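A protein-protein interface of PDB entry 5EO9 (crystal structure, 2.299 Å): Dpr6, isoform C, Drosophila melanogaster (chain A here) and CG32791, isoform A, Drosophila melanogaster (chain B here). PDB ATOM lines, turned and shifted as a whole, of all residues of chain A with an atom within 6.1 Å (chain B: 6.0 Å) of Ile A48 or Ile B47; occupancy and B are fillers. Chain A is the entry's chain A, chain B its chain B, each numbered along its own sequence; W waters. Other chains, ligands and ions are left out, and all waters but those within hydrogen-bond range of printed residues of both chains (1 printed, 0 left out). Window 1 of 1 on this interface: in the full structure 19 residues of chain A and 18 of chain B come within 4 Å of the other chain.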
ATOM      1  N   SER A  39     -14.753   4.570  33.041  1.00  0.00           N
ATOM      2  CA  SER A  39     -13.761   5.328  32.299  1.00  0.00           C
ATOM      3  C   SER A  39     -14.411   6.494  31.570  1.00  0.00           C
ATOM      4  O   SER A  39     -15.555   6.403  31.124  1.00  0.00           O
ATOM      5  CB  SER A  39     -13.032   4.443  31.279  1.00  0.00           C
ATOM      6  OG  SER A  39     -12.208   3.494  31.918  1.00  0.00           O
ATOM      7  N   TRP A  40     -13.639   7.569  31.413  1.00  0.00           N
ATOM      8  CA  TRP A  40     -14.027   8.748  30.653  1.00  0.00           C
ATOM      9  C   TRP A  40     -13.253   8.806  29.340  1.00  0.00           C
ATOM     10  O   TRP A  40     -12.020   8.679  29.321  1.00  0.00           O
ATOM     11  CB  TRP A  40     -13.784  10.024  31.461  1.00  0.00           C
ATOM     12  CG  TRP A  40     -14.867  10.312  32.444  1.00  0.00           C
ATOM     13  CD1 TRP A  40     -14.816  10.139  33.789  1.00  0.00           C
ATOM     14  CD2 TRP A  40     -16.170  10.826  32.151  1.00  0.00           C
ATOM     15  NE1 TRP A  40     -16.004  10.521  34.362  1.00  0.00           N
ATOM     16  CE2 TRP A  40     -16.854  10.945  33.375  1.00  0.00           C
ATOM     17  CE3 TRP A  40     -16.824  11.205  30.967  1.00  0.00           C
ATOM     18  CZ2 TRP A  40     -18.157  11.424  33.455  1.00  0.00           C
ATOM     19  CZ3 TRP A  40     -18.110  11.670  31.046  1.00  0.00           C
ATOM     20  CH2 TRP A  40     -18.767  11.784  32.281  1.00  0.00           C
ATOM     21  N   ILE A  41     -13.982   9.008  28.248  1.00  0.00           N
ATOM     22  CA  ILE A  41     -13.404   9.083  26.916  1.00  0.00           C
ATOM     23  C   ILE A  41     -13.898  10.355  26.241  1.00  0.00           C
ATOM     24  O   ILE A  41     -15.085  10.688  26.327  1.00  0.00           O
ATOM     25  CB  ILE A  41     -13.776   7.848  26.079  1.00  0.00           C
ATOM     26  CG1 ILE A  41     -13.302   6.576  26.793  1.00  0.00           C
ATOM     27  CG2 ILE A  41     -13.216   7.960  24.683  1.00  0.00           C
ATOM     28  CD1 ILE A  41     -13.906   5.311  26.250  1.00  0.00           C
ATOM     29  N   ARG A  42     -12.985  11.054  25.564  1.00  0.00           N
ATOM     30  CA  ARG A  42     -13.306  12.232  24.776  1.00  0.00           C
ATOM     31  C   ARG A  42     -13.543  11.830  23.327  1.00  0.00           C
ATOM     32  O   ARG A  42     -12.667  11.239  22.694  1.00  0.00           O
ATOM     33  CB  ARG A  42     -12.170  13.249  24.869  1.00  0.00           C
ATOM     34  CG  ARG A  42     -12.358  14.480  23.999  1.00  0.00           C
ATOM     35  CD  ARG A  42     -11.026  14.948  23.490  1.00  0.00           C
ATOM     36  NE  ARG A  42     -10.333  15.804  24.438  1.00  0.00           N
ATOM     37  CZ  ARG A  42      -9.011  15.892  24.542  1.00  0.00           C
ATOM     38  NH1 ARG A  42      -8.225  15.147  23.773  1.00  0.00           N
ATOM     39  NH2 ARG A  42      -8.475  16.726  25.426  1.00  0.00           N
ATOM     40  N   ILE A  46     -11.299  10.197  20.250  1.00  0.00           N
ATOM     41  CA  ILE A  46     -11.394   8.931  20.976  1.00  0.00           C
ATOM     42  C   ILE A  46     -10.232   8.793  21.954  1.00  0.00           C
ATOM     43  O   ILE A  46      -9.672   7.703  22.133  1.00  0.00           O
ATOM     44  CB  ILE A  46     -11.471   7.731  20.010  1.00  0.00           C
ATOM     45  CG1 ILE A  46     -12.336   8.079  18.801  1.00  0.00           C
ATOM     46  CG2 ILE A  46     -12.086   6.519  20.702  1.00  0.00           C
ATOM     47  CD1 ILE A  46     -12.593   6.906  17.882  1.00  0.00           C
ATOM     48  N   HIS A  47      -9.874   9.891  22.612  1.00  0.00           N
ATOM     49  CA  HIS A  47      -8.762   9.886  23.554  1.00  0.00           C
ATOM     50  C   HIS A  47      -9.230   9.361  24.903  1.00  0.00           C
ATOM     51  O   HIS A  47     -10.159   9.916  25.501  1.00  0.00           O
ATOM     52  CB  HIS A  47      -8.164  11.280  23.715  1.00  0.00           C
ATOM     53  CG  HIS A  47      -6.955  11.307  24.596  1.00  0.00           C
ATOM     54  ND1 HIS A  47      -6.190  10.185  24.838  1.00  0.00           N
ATOM     55  CD2 HIS A  47      -6.382  12.314  25.299  1.00  0.00           C
ATOM     56  CE1 HIS A  47      -5.196  10.501  25.650  1.00  0.00           C
ATOM     57  NE2 HIS A  47      -5.295  11.785  25.951  1.00  0.00           N
ATOM     58  N   ILE A  48      -8.586   8.297  25.386  1.00  0.00           N
ATOM     59  CA  ILE A  48      -8.869   7.817  26.736  1.00  0.00           C
ATOM     60  C   ILE A  48      -8.359   8.832  27.748  1.00  0.00           C
ATOM     61  O   ILE A  48      -7.183   9.216  27.729  1.00  0.00           O
ATOM     62  CB  ILE A  48      -8.226   6.448  26.984  1.00  0.00           C
ATOM     63  CG1 ILE A  48      -8.754   5.408  25.991  1.00  0.00           C
ATOM     64  CG2 ILE A  48      -8.475   6.034  28.430  1.00  0.00           C
ATOM     65  CD1 ILE A  48      -7.996   4.082  26.022  1.00  0.00           C
ATOM     66  N   LEU A  49      -9.237   9.256  28.654  1.00  0.00           N
ATOM     67  CA  LEU A  49      -8.883  10.275  29.638  1.00  0.00           C
ATOM     68  C   LEU A  49      -8.524   9.639  30.975  1.00  0.00           C
ATOM     69  O   LEU A  49      -7.395   9.783  31.457  1.00  0.00           O
ATOM     70  CB  LEU A  49     -10.038  11.294  29.793  1.00  0.00           C
ATOM     71  CG  LEU A  49     -10.451  11.992  28.475  1.00  0.00           C
ATOM     72  CD1 LEU A  49     -11.581  13.028  28.646  1.00  0.00           C
ATOM     73  CD2 LEU A  49      -9.241  12.654  27.800  1.00  0.00           C
ATOM     74  N   THR A  50      -9.464   8.910  31.567  1.00  0.00           N
ATOM     75  CA  THR A  50      -9.283   8.305  32.875  1.00  0.00           C
ATOM     76  C   THR A  50      -9.872   6.898  32.875  1.00  0.00           C
ATOM     77  O   THR A  50     -10.805   6.594  32.125  1.00  0.00           O
ATOM     78  CB  THR A  50      -9.951   9.144  33.981  1.00  0.00           C
ATOM     79  OG1 THR A  50     -11.354   9.246  33.728  1.00  0.00           O
ATOM     80  CG2 THR A  50      -9.366  10.546  34.038  1.00  0.00           C
ATOM     81  N   VAL A  51      -9.328   6.049  33.737  1.00  0.00           N
ATOM     82  CA  VAL A  51      -9.876   4.717  33.993  1.00  0.00           C
ATOM     83  C   VAL A  51      -9.998   4.594  35.503  1.00  0.00           C
ATOM     84  O   VAL A  51      -8.988   4.456  36.201  1.00  0.00           O
ATOM     85  CB  VAL A  51      -9.006   3.598  33.415  1.00  0.00           C
ATOM     86  CG1 VAL A  51      -9.551   2.242  33.839  1.00  0.00           C
ATOM     87  CG2 VAL A  51      -8.944   3.713  31.906  1.00  0.00           C
ATOM     88  N   TYR A  56      -4.994   8.550  32.488  1.00  0.00           N
ATOM     89  CA  TYR A  56      -4.214   8.189  31.311  1.00  0.00           C
ATOM     90  C   TYR A  56      -3.685   9.403  30.555  1.00  0.00           C
ATOM     91  O   TYR A  56      -2.495   9.456  30.235  1.00  0.00           O
ATOM     92  CB  TYR A  56      -5.059   7.317  30.379  1.00  0.00           C
ATOM     93  CG  TYR A  56      -4.345   6.880  29.121  1.00  0.00           C
ATOM     94  CD1 TYR A  56      -3.260   6.021  29.180  1.00  0.00           C
ATOM     95  CD2 TYR A  56      -4.778   7.311  27.870  1.00  0.00           C
ATOM     96  CE1 TYR A  56      -2.615   5.605  28.026  1.00  0.00           C
ATOM     97  CE2 TYR A  56      -4.146   6.916  26.715  1.00  0.00           C
ATOM     98  CZ  TYR A  56      -3.061   6.049  26.795  1.00  0.00           C
ATOM     99  OH  TYR A  56      -2.413   5.631  25.652  1.00  0.00           O
ATOM    100  N   THR A  57      -4.540  10.383  30.257  1.00  0.00           N
ATOM    101  CA  THR A  57      -4.100  11.520  29.456  1.00  0.00           C
ATOM    102  C   THR A  57      -2.942  12.252  30.132  1.00  0.00           C
ATOM    103  O   THR A  57      -2.841  12.301  31.359  1.00  0.00           O
ATOM    104  CB  THR A  57      -5.261  12.490  29.207  1.00  0.00           C
ATOM    105  OG1 THR A  57      -4.757  13.684  28.602  1.00  0.00           O
ATOM    106  CG2 THR A  57      -5.968  12.860  30.512  1.00  0.00           C
ATOM    107  N   GLN A  91     -17.917   5.289  30.459  1.00  0.00           N
ATOM    108  CA  GLN A  91     -17.927   3.929  29.921  1.00  0.00           C
ATOM    109  C   GLN A  91     -17.643   2.893  31.001  1.00  0.00           C
ATOM    110  O   GLN A  91     -16.603   2.951  31.669  1.00  0.00           O
ATOM    111  CB  GLN A  91     -16.902   3.786  28.794  1.00  0.00           C
ATOM    112  CG  GLN A  91     -16.958   2.469  28.061  1.00  0.00           C
ATOM    113  CD  GLN A  91     -15.836   2.319  27.048  1.00  0.00           C
ATOM    114  OE1 GLN A  91     -14.812   1.703  27.336  1.00  0.00           O
ATOM    115  NE2 GLN A  91     -16.031   2.863  25.851  1.00  0.00           N
ATOM    116  N   SER A  93     -16.820  -0.988  31.990  1.00  0.00           N
ATOM    117  CA  SER A  93     -16.054  -2.073  31.374  1.00  0.00           C
ATOM    118  C   SER A  93     -16.768  -3.419  31.393  1.00  0.00           C
ATOM    119  O   SER A  93     -16.124  -4.453  31.582  1.00  0.00           O
ATOM    120  CB  SER A  93     -14.689  -2.184  32.054  1.00  0.00           C
ATOM    121  OG  SER A  93     -14.788  -2.725  33.357  1.00  0.00           O
ATOM    122  N   VAL A  97     -19.186  -3.189  26.386  1.00  0.00           N
ATOM    123  CA  VAL A  97     -19.173  -2.025  27.264  1.00  0.00           C
ATOM    124  C   VAL A  97     -20.530  -1.335  27.262  1.00  0.00           C
ATOM    125  O   VAL A  97     -21.276  -1.360  26.272  1.00  0.00           O
ATOM    126  CB  VAL A  97     -18.074  -1.024  26.865  1.00  0.00           C
ATOM    127  CG1 VAL A  97     -16.693  -1.604  27.117  1.00  0.00           C
ATOM    128  CG2 VAL A  97     -18.258  -0.585  25.413  1.00  0.00           C
ATOM    129  N   GLY B  38      -2.216   2.376  24.836  1.00  0.00           N
ATOM    130  CA  GLY B  38      -3.601   2.018  25.076  1.00  0.00           C
ATOM    131  C   GLY B  38      -4.186   1.335  23.851  1.00  0.00           C
ATOM    132  O   GLY B  38      -3.772   1.603  22.722  1.00  0.00           O
ATOM    133  N   TRP B  39      -5.146   0.439  24.078  1.00  0.00           N
ATOM    134  CA  TRP B  39      -5.863  -0.231  23.001  1.00  0.00           C
ATOM    135  C   TRP B  39      -7.360  -0.051  23.191  1.00  0.00           C
ATOM    136  O   TRP B  39      -7.864  -0.188  24.309  1.00  0.00           O
ATOM    137  CB  TRP B  39      -5.565  -1.736  22.963  1.00  0.00           C
ATOM    138  CG  TRP B  39      -4.237  -2.108  22.438  1.00  0.00           C
ATOM    139  CD1 TRP B  39      -3.151  -2.480  23.165  1.00  0.00           C
ATOM    140  CD2 TRP B  39      -3.848  -2.175  21.064  1.00  0.00           C
ATOM    141  NE1 TRP B  39      -2.100  -2.772  22.332  1.00  0.00           N
ATOM    142  CE2 TRP B  39      -2.502  -2.598  21.034  1.00  0.00           C
ATOM    143  CE3 TRP B  39      -4.509  -1.930  19.857  1.00  0.00           C
ATOM    144  CZ2 TRP B  39      -1.798  -2.779  19.843  1.00  0.00           C
ATOM    145  CZ3 TRP B  39      -3.812  -2.101  18.675  1.00  0.00           C
ATOM    146  CH2 TRP B  39      -2.465  -2.520  18.676  1.00  0.00           C
ATOM    147  N   LEU B  40      -8.078   0.209  22.099  1.00  0.00           N
ATOM    148  CA  LEU B  40      -9.533   0.179  22.178  1.00  0.00           C
ATOM    149  C   LEU B  40     -10.118  -0.210  20.824  1.00  0.00           C
ATOM    150  O   LEU B  40      -9.458  -0.096  19.789  1.00  0.00           O
ATOM    151  CB  LEU B  40     -10.091   1.526  22.659  1.00  0.00           C
ATOM    152  CG  LEU B  40      -9.745   2.810  21.896  1.00  0.00           C
ATOM    153  CD1 LEU B  40     -10.519   2.938  20.586  1.00  0.00           C
ATOM    154  CD2 LEU B  40      -9.990   4.038  22.786  1.00  0.00           C
ATOM    155  N   LYS B  41     -11.378  -0.664  20.853  1.00  0.00           N
ATOM    156  CA  LYS B  41     -12.148  -0.929  19.640  1.00  0.00           C
ATOM    157  C   LYS B  41     -12.686   0.384  19.073  1.00  0.00           C
ATOM    158  O   LYS B  41     -13.468   1.072  19.734  1.00  0.00           O
ATOM    159  CB  LYS B  41     -13.312  -1.881  19.926  1.00  0.00           C
ATOM    160  CG  LYS B  41     -12.926  -3.244  20.485  1.00  0.00           C
ATOM    161  CD  LYS B  41     -14.127  -4.187  20.503  1.00  0.00           C
ATOM    162  CE  LYS B  41     -14.684  -4.373  19.091  1.00  0.00           C
ATOM    163  NZ  LYS B  41     -15.790  -5.374  19.018  1.00  0.00           N
ATOM    164  N   LYS B  45     -15.653   2.170  20.784  1.00  0.00           N
ATOM    165  CA  LYS B  45     -14.810   2.920  21.708  1.00  0.00           C
ATOM    166  C   LYS B  45     -14.476   2.119  22.962  1.00  0.00           C
ATOM    167  O   LYS B  45     -13.894   2.665  23.904  1.00  0.00           O
ATOM    168  CB  LYS B  45     -15.443   4.268  22.077  1.00  0.00           C
ATOM    169  CG  LYS B  45     -15.873   5.102  20.874  1.00  0.00           C
ATOM    170  CD  LYS B  45     -16.279   6.521  21.301  1.00  0.00           C
ATOM    171  CE  LYS B  45     -16.752   7.358  20.114  1.00  0.00           C
ATOM    172  NZ  LYS B  45     -17.922   6.751  19.418  1.00  0.00           N
ATOM    173  N   ALA B  46     -14.823   0.832  22.988  1.00  0.00           N
ATOM    174  CA  ALA B  46     -14.576  -0.004  24.153  1.00  0.00           C
ATOM    175  C   ALA B  46     -13.085  -0.054  24.444  1.00  0.00           C
ATOM    176  O   ALA B  46     -12.288  -0.422  23.578  1.00  0.00           O
ATOM    177  CB  ALA B  46     -15.120  -1.412  23.919  1.00  0.00           C
ATOM    178  N   ILE B  47     -12.708   0.334  25.658  1.00  0.00           N
ATOM    179  CA  ILE B  47     -11.307   0.278  26.057  1.00  0.00           C
ATOM    180  C   ILE B  47     -10.906  -1.173  26.279  1.00  0.00           C
ATOM    181  O   ILE B  47     -11.588  -1.920  26.992  1.00  0.00           O
ATOM    182  CB  ILE B  47     -11.080   1.109  27.323  1.00  0.00           C
ATOM    183  CG1 ILE B  47     -11.460   2.582  27.071  1.00  0.00           C
ATOM    184  CG2 ILE B  47      -9.644   0.948  27.805  1.00  0.00           C
ATOM    185  CD1 ILE B  47     -11.194   3.471  28.257  1.00  0.00           C
ATOM    186  N   GLN B  48      -9.797  -1.582  25.669  1.00  0.00           N
ATOM    187  CA  GLN B  48      -9.343  -2.963  25.795  1.00  0.00           C
ATOM    188  C   GLN B  48      -8.280  -3.121  26.872  1.00  0.00           C
ATOM    189  O   GLN B  48      -8.396  -3.995  27.741  1.00  0.00           O
ATOM    190  CB  GLN B  48      -8.810  -3.473  24.453  1.00  0.00           C
ATOM    191  CG  GLN B  48      -9.842  -3.434  23.351  1.00  0.00           C
ATOM    192  CD  GLN B  48     -11.075  -4.240  23.701  1.00  0.00           C
ATOM    193  OE1 GLN B  48     -11.012  -5.473  23.816  1.00  0.00           O
ATOM    194  NE2 GLN B  48     -12.205  -3.556  23.880  1.00  0.00           N
ATOM    195  N   ALA B  49      -7.270  -2.259  26.855  1.00  0.00           N
ATOM    196  CA  ALA B  49      -6.141  -2.408  27.754  1.00  0.00           C
ATOM    197  C   ALA B  49      -5.319  -1.131  27.747  1.00  0.00           C
ATOM    198  O   ALA B  49      -5.295  -0.386  26.761  1.00  0.00           O
ATOM    199  CB  ALA B  49      -5.261  -3.599  27.352  1.00  0.00           C
ATOM    200  N   ILE B  50      -4.625  -0.905  28.860  1.00  0.00           N
ATOM    201  CA  ILE B  50      -3.627   0.146  28.969  1.00  0.00           C
ATOM    202  C   ILE B  50      -2.374  -0.448  29.588  1.00  0.00           C
ATOM    203  O   ILE B  50      -2.414  -0.959  30.715  1.00  0.00           O
ATOM    204  CB  ILE B  50      -4.108   1.333  29.810  1.00  0.00           C
ATOM    205  CG1 ILE B  50      -5.282   2.031  29.124  1.00  0.00           C
ATOM    206  CG2 ILE B  50      -2.941   2.286  30.044  1.00  0.00           C
ATOM    207  CD1 ILE B  50      -5.897   3.110  29.973  1.00  0.00           C
ATOM    208  N   ILE B  55      -8.364  -4.067  30.475  1.00  0.00           N
ATOM    209  CA  ILE B  55      -9.479  -3.362  31.081  1.00  0.00           C
ATOM    210  C   ILE B  55     -10.809  -4.004  30.719  1.00  0.00           C
ATOM    211  O   ILE B  55     -11.713  -4.064  31.552  1.00  0.00           O
ATOM    212  CB  ILE B  55      -9.443  -1.866  30.699  1.00  0.00           C
ATOM    213  CG1 ILE B  55      -8.195  -1.231  31.320  1.00  0.00           C
ATOM    214  CG2 ILE B  55     -10.725  -1.161  31.157  1.00  0.00           C
ATOM    215  CD1 ILE B  55      -7.951   0.180  30.903  1.00  0.00           C
ATOM    216  N   THR B  56     -10.943  -4.498  29.494  1.00  0.00           N
ATOM    217  CA  THR B  56     -12.172  -5.174  29.120  1.00  0.00           C
ATOM    218  C   THR B  56     -12.338  -6.460  29.919  1.00  0.00           C
ATOM    219  O   THR B  56     -11.363  -7.130  30.263  1.00  0.00           O
ATOM    220  CB  THR B  56     -12.197  -5.475  27.624  1.00  0.00           C
ATOM    221  OG1 THR B  56     -13.423  -6.144  27.317  1.00  0.00           O
ATOM    222  CG2 THR B  56     -11.016  -6.348  27.208  1.00  0.00           C
ATOM    223  N   GLN B  89      -3.044   3.611  20.927  1.00  0.00           N
ATOM    224  CA  GLN B  89      -3.076   4.992  21.378  1.00  0.00           C
ATOM    225  C   GLN B  89      -1.942   5.221  22.365  1.00  0.00           C
ATOM    226  O   GLN B  89      -1.664   4.362  23.208  1.00  0.00           O
ATOM    227  CB  GLN B  89      -4.449   5.293  22.005  1.00  0.00           C
ATOM    228  CG  GLN B  89      -4.593   6.629  22.689  1.00  0.00           C
ATOM    229  CD  GLN B  89      -6.010   6.863  23.204  1.00  0.00           C
ATOM    230  OE1 GLN B  89      -6.210   7.526  24.217  1.00  0.00           O
ATOM    231  NE2 GLN B  89      -6.997   6.327  22.495  1.00  0.00           N
ATOM    232  N   MET B  95      -2.385  13.456  22.007  1.00  0.00           N
ATOM    233  CA  MET B  95      -2.356  12.008  21.869  1.00  0.00           C
ATOM    234  C   MET B  95      -2.064  11.608  20.428  1.00  0.00           C
ATOM    235  O   MET B  95      -2.393  12.328  19.481  1.00  0.00           O
ATOM    236  CB  MET B  95      -3.687  11.392  22.321  1.00  0.00           C
ATOM    237  CG  MET B  95      -4.897  11.793  21.472  1.00  0.00           C
ATOM    238  SD  MET B  95      -5.341  10.622  20.160  1.00  0.00           S
ATOM    239  CE  MET B  95      -6.279   9.412  21.082  1.00  0.00           C
HETATM  240  O   HOH W   1     -11.986  -2.915  34.090  1.00  0.00           O
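OE1 of Gln B89 is in hydrogen-bond range of ND1 of His A47 (2.7 Å). O of Ile A46 lies within hydrogen-bond range of NE2 of Gln B89 (3.0 Å). OE1 of Gln A91 sits at hydrogen-bond distance from N of Ile B47 (3.0 Å). N of Ile A48 is in hydrogen-bond range of OE1 of Gln B89 (2.8 Å). The backbone carbonyl oxygen of Lys B45 sits at hydrogen-bond distance from the side-chain amide nitrogen of Gln A91. The side-chain hydroxyl (OH) of Tyr A56 is in hydrogen-bond range of the backbone carbonyl oxygen (O) of Gln B89 (2.9 Å). N of Gly B38 is in hydrogen-bond range of OH of Tyr A56, at 3.4 Å.
Along chain A the printed residues that touch a printed residue of chain B span positions 39 to 97. Printed residues of chain B that touch a printed residue of chain A: Gly B38, Leu B40, Lys B45, Ala B46, Ile B47, Ile B50, Ile B55, Gln B89 and Met B95. Hydrophobic or aromatic side chains of chain B within 4 Å of the printed part of chain A: Leu B40, Ala B46, Ile B47, Ile B50, Ile B55 and Met B95. Among the printed residues, no Asp or Glu carboxylate lies within 4 Å of a Lys or Arg side-chain nitrogen of the other chain.
Arg A42 touches none of the printed residues of chain B. Leu A49 touches none of the printed residues of chain B. Of the printed residues of chain B, Gln A91 touches Lys B45 (2.9 Å), Ala B46 (3.6 Å) and Ile B47 (3.0 Å). Printed residues of chain B within 4 Å of Val A97: Ala B46. Printed residues of chain A within 4 Å of Leu B40: Ile A46 (3.7 Å) and Ile A48 (3.7 Å). Ile B47 touches four residues of chain A. Of the printed residues of chain A, Gln B89 touches Ile A46, His A47, Ile A48 and Tyr A56. The nearest printed residue of chain B that does not touch Val A97 is Ile B47 (4.7 Å).
NE2 of His A47 sits at hydrogen-bond distance from OG1 of Thr A57 (3.3 Å). The backbone carbonyl oxygen of His A47 lies within hydrogen-bond range of the backbone NH of Arg A42, at 3.0 Å. The backbone carbonyl oxygen (O) of Gln B48 lies within hydrogen-bond range of the backbone NH (N) of Ile B55 (2.7 Å). The side-chain hydroxyl (OG) of Ser A39 sits close to the backbone carbonyl oxygen (O) of Thr A50. The backbone carbonyl oxygen (O) of Ala B46 sits at hydrogen-bond distance from the backbone NH (N) of Lys B41 (2.9 Å). N of Gly B38 sits at hydrogen-bond distance from O of Gln B89 (2.6 Å).
CD1 of Ile B47 touches CB of Ser A39, 3.7 Å away. O of Lys B45 touches CD1 of Ile A41, at 3.5 Å. CG1 of Ile B47 touches CD1 of Ile A41 (3.8 Å). Ile A46 touches Leu B40 (O to CD2, 3.7 Å). His A47 touches Met B95 (CA to CE, 3.5 Å). CD1 of Ile B47 touches CG2 of Ile A48 (3.7 Å). Ile B50 touches Val A51. Val A51 touches Ile B55 (CG2 to CD1, 3.8 Å). Ile B50 touches Tyr A56 (CG2 to CD1, 3.8 Å). Val A97 touches Ala B46.
Water W1 bridges the backbone carbonyl oxygen (O) of Ile B55 (2.8 Å) and the side-chain hydroxyl (OG) of Ser A93 (2.9 Å).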
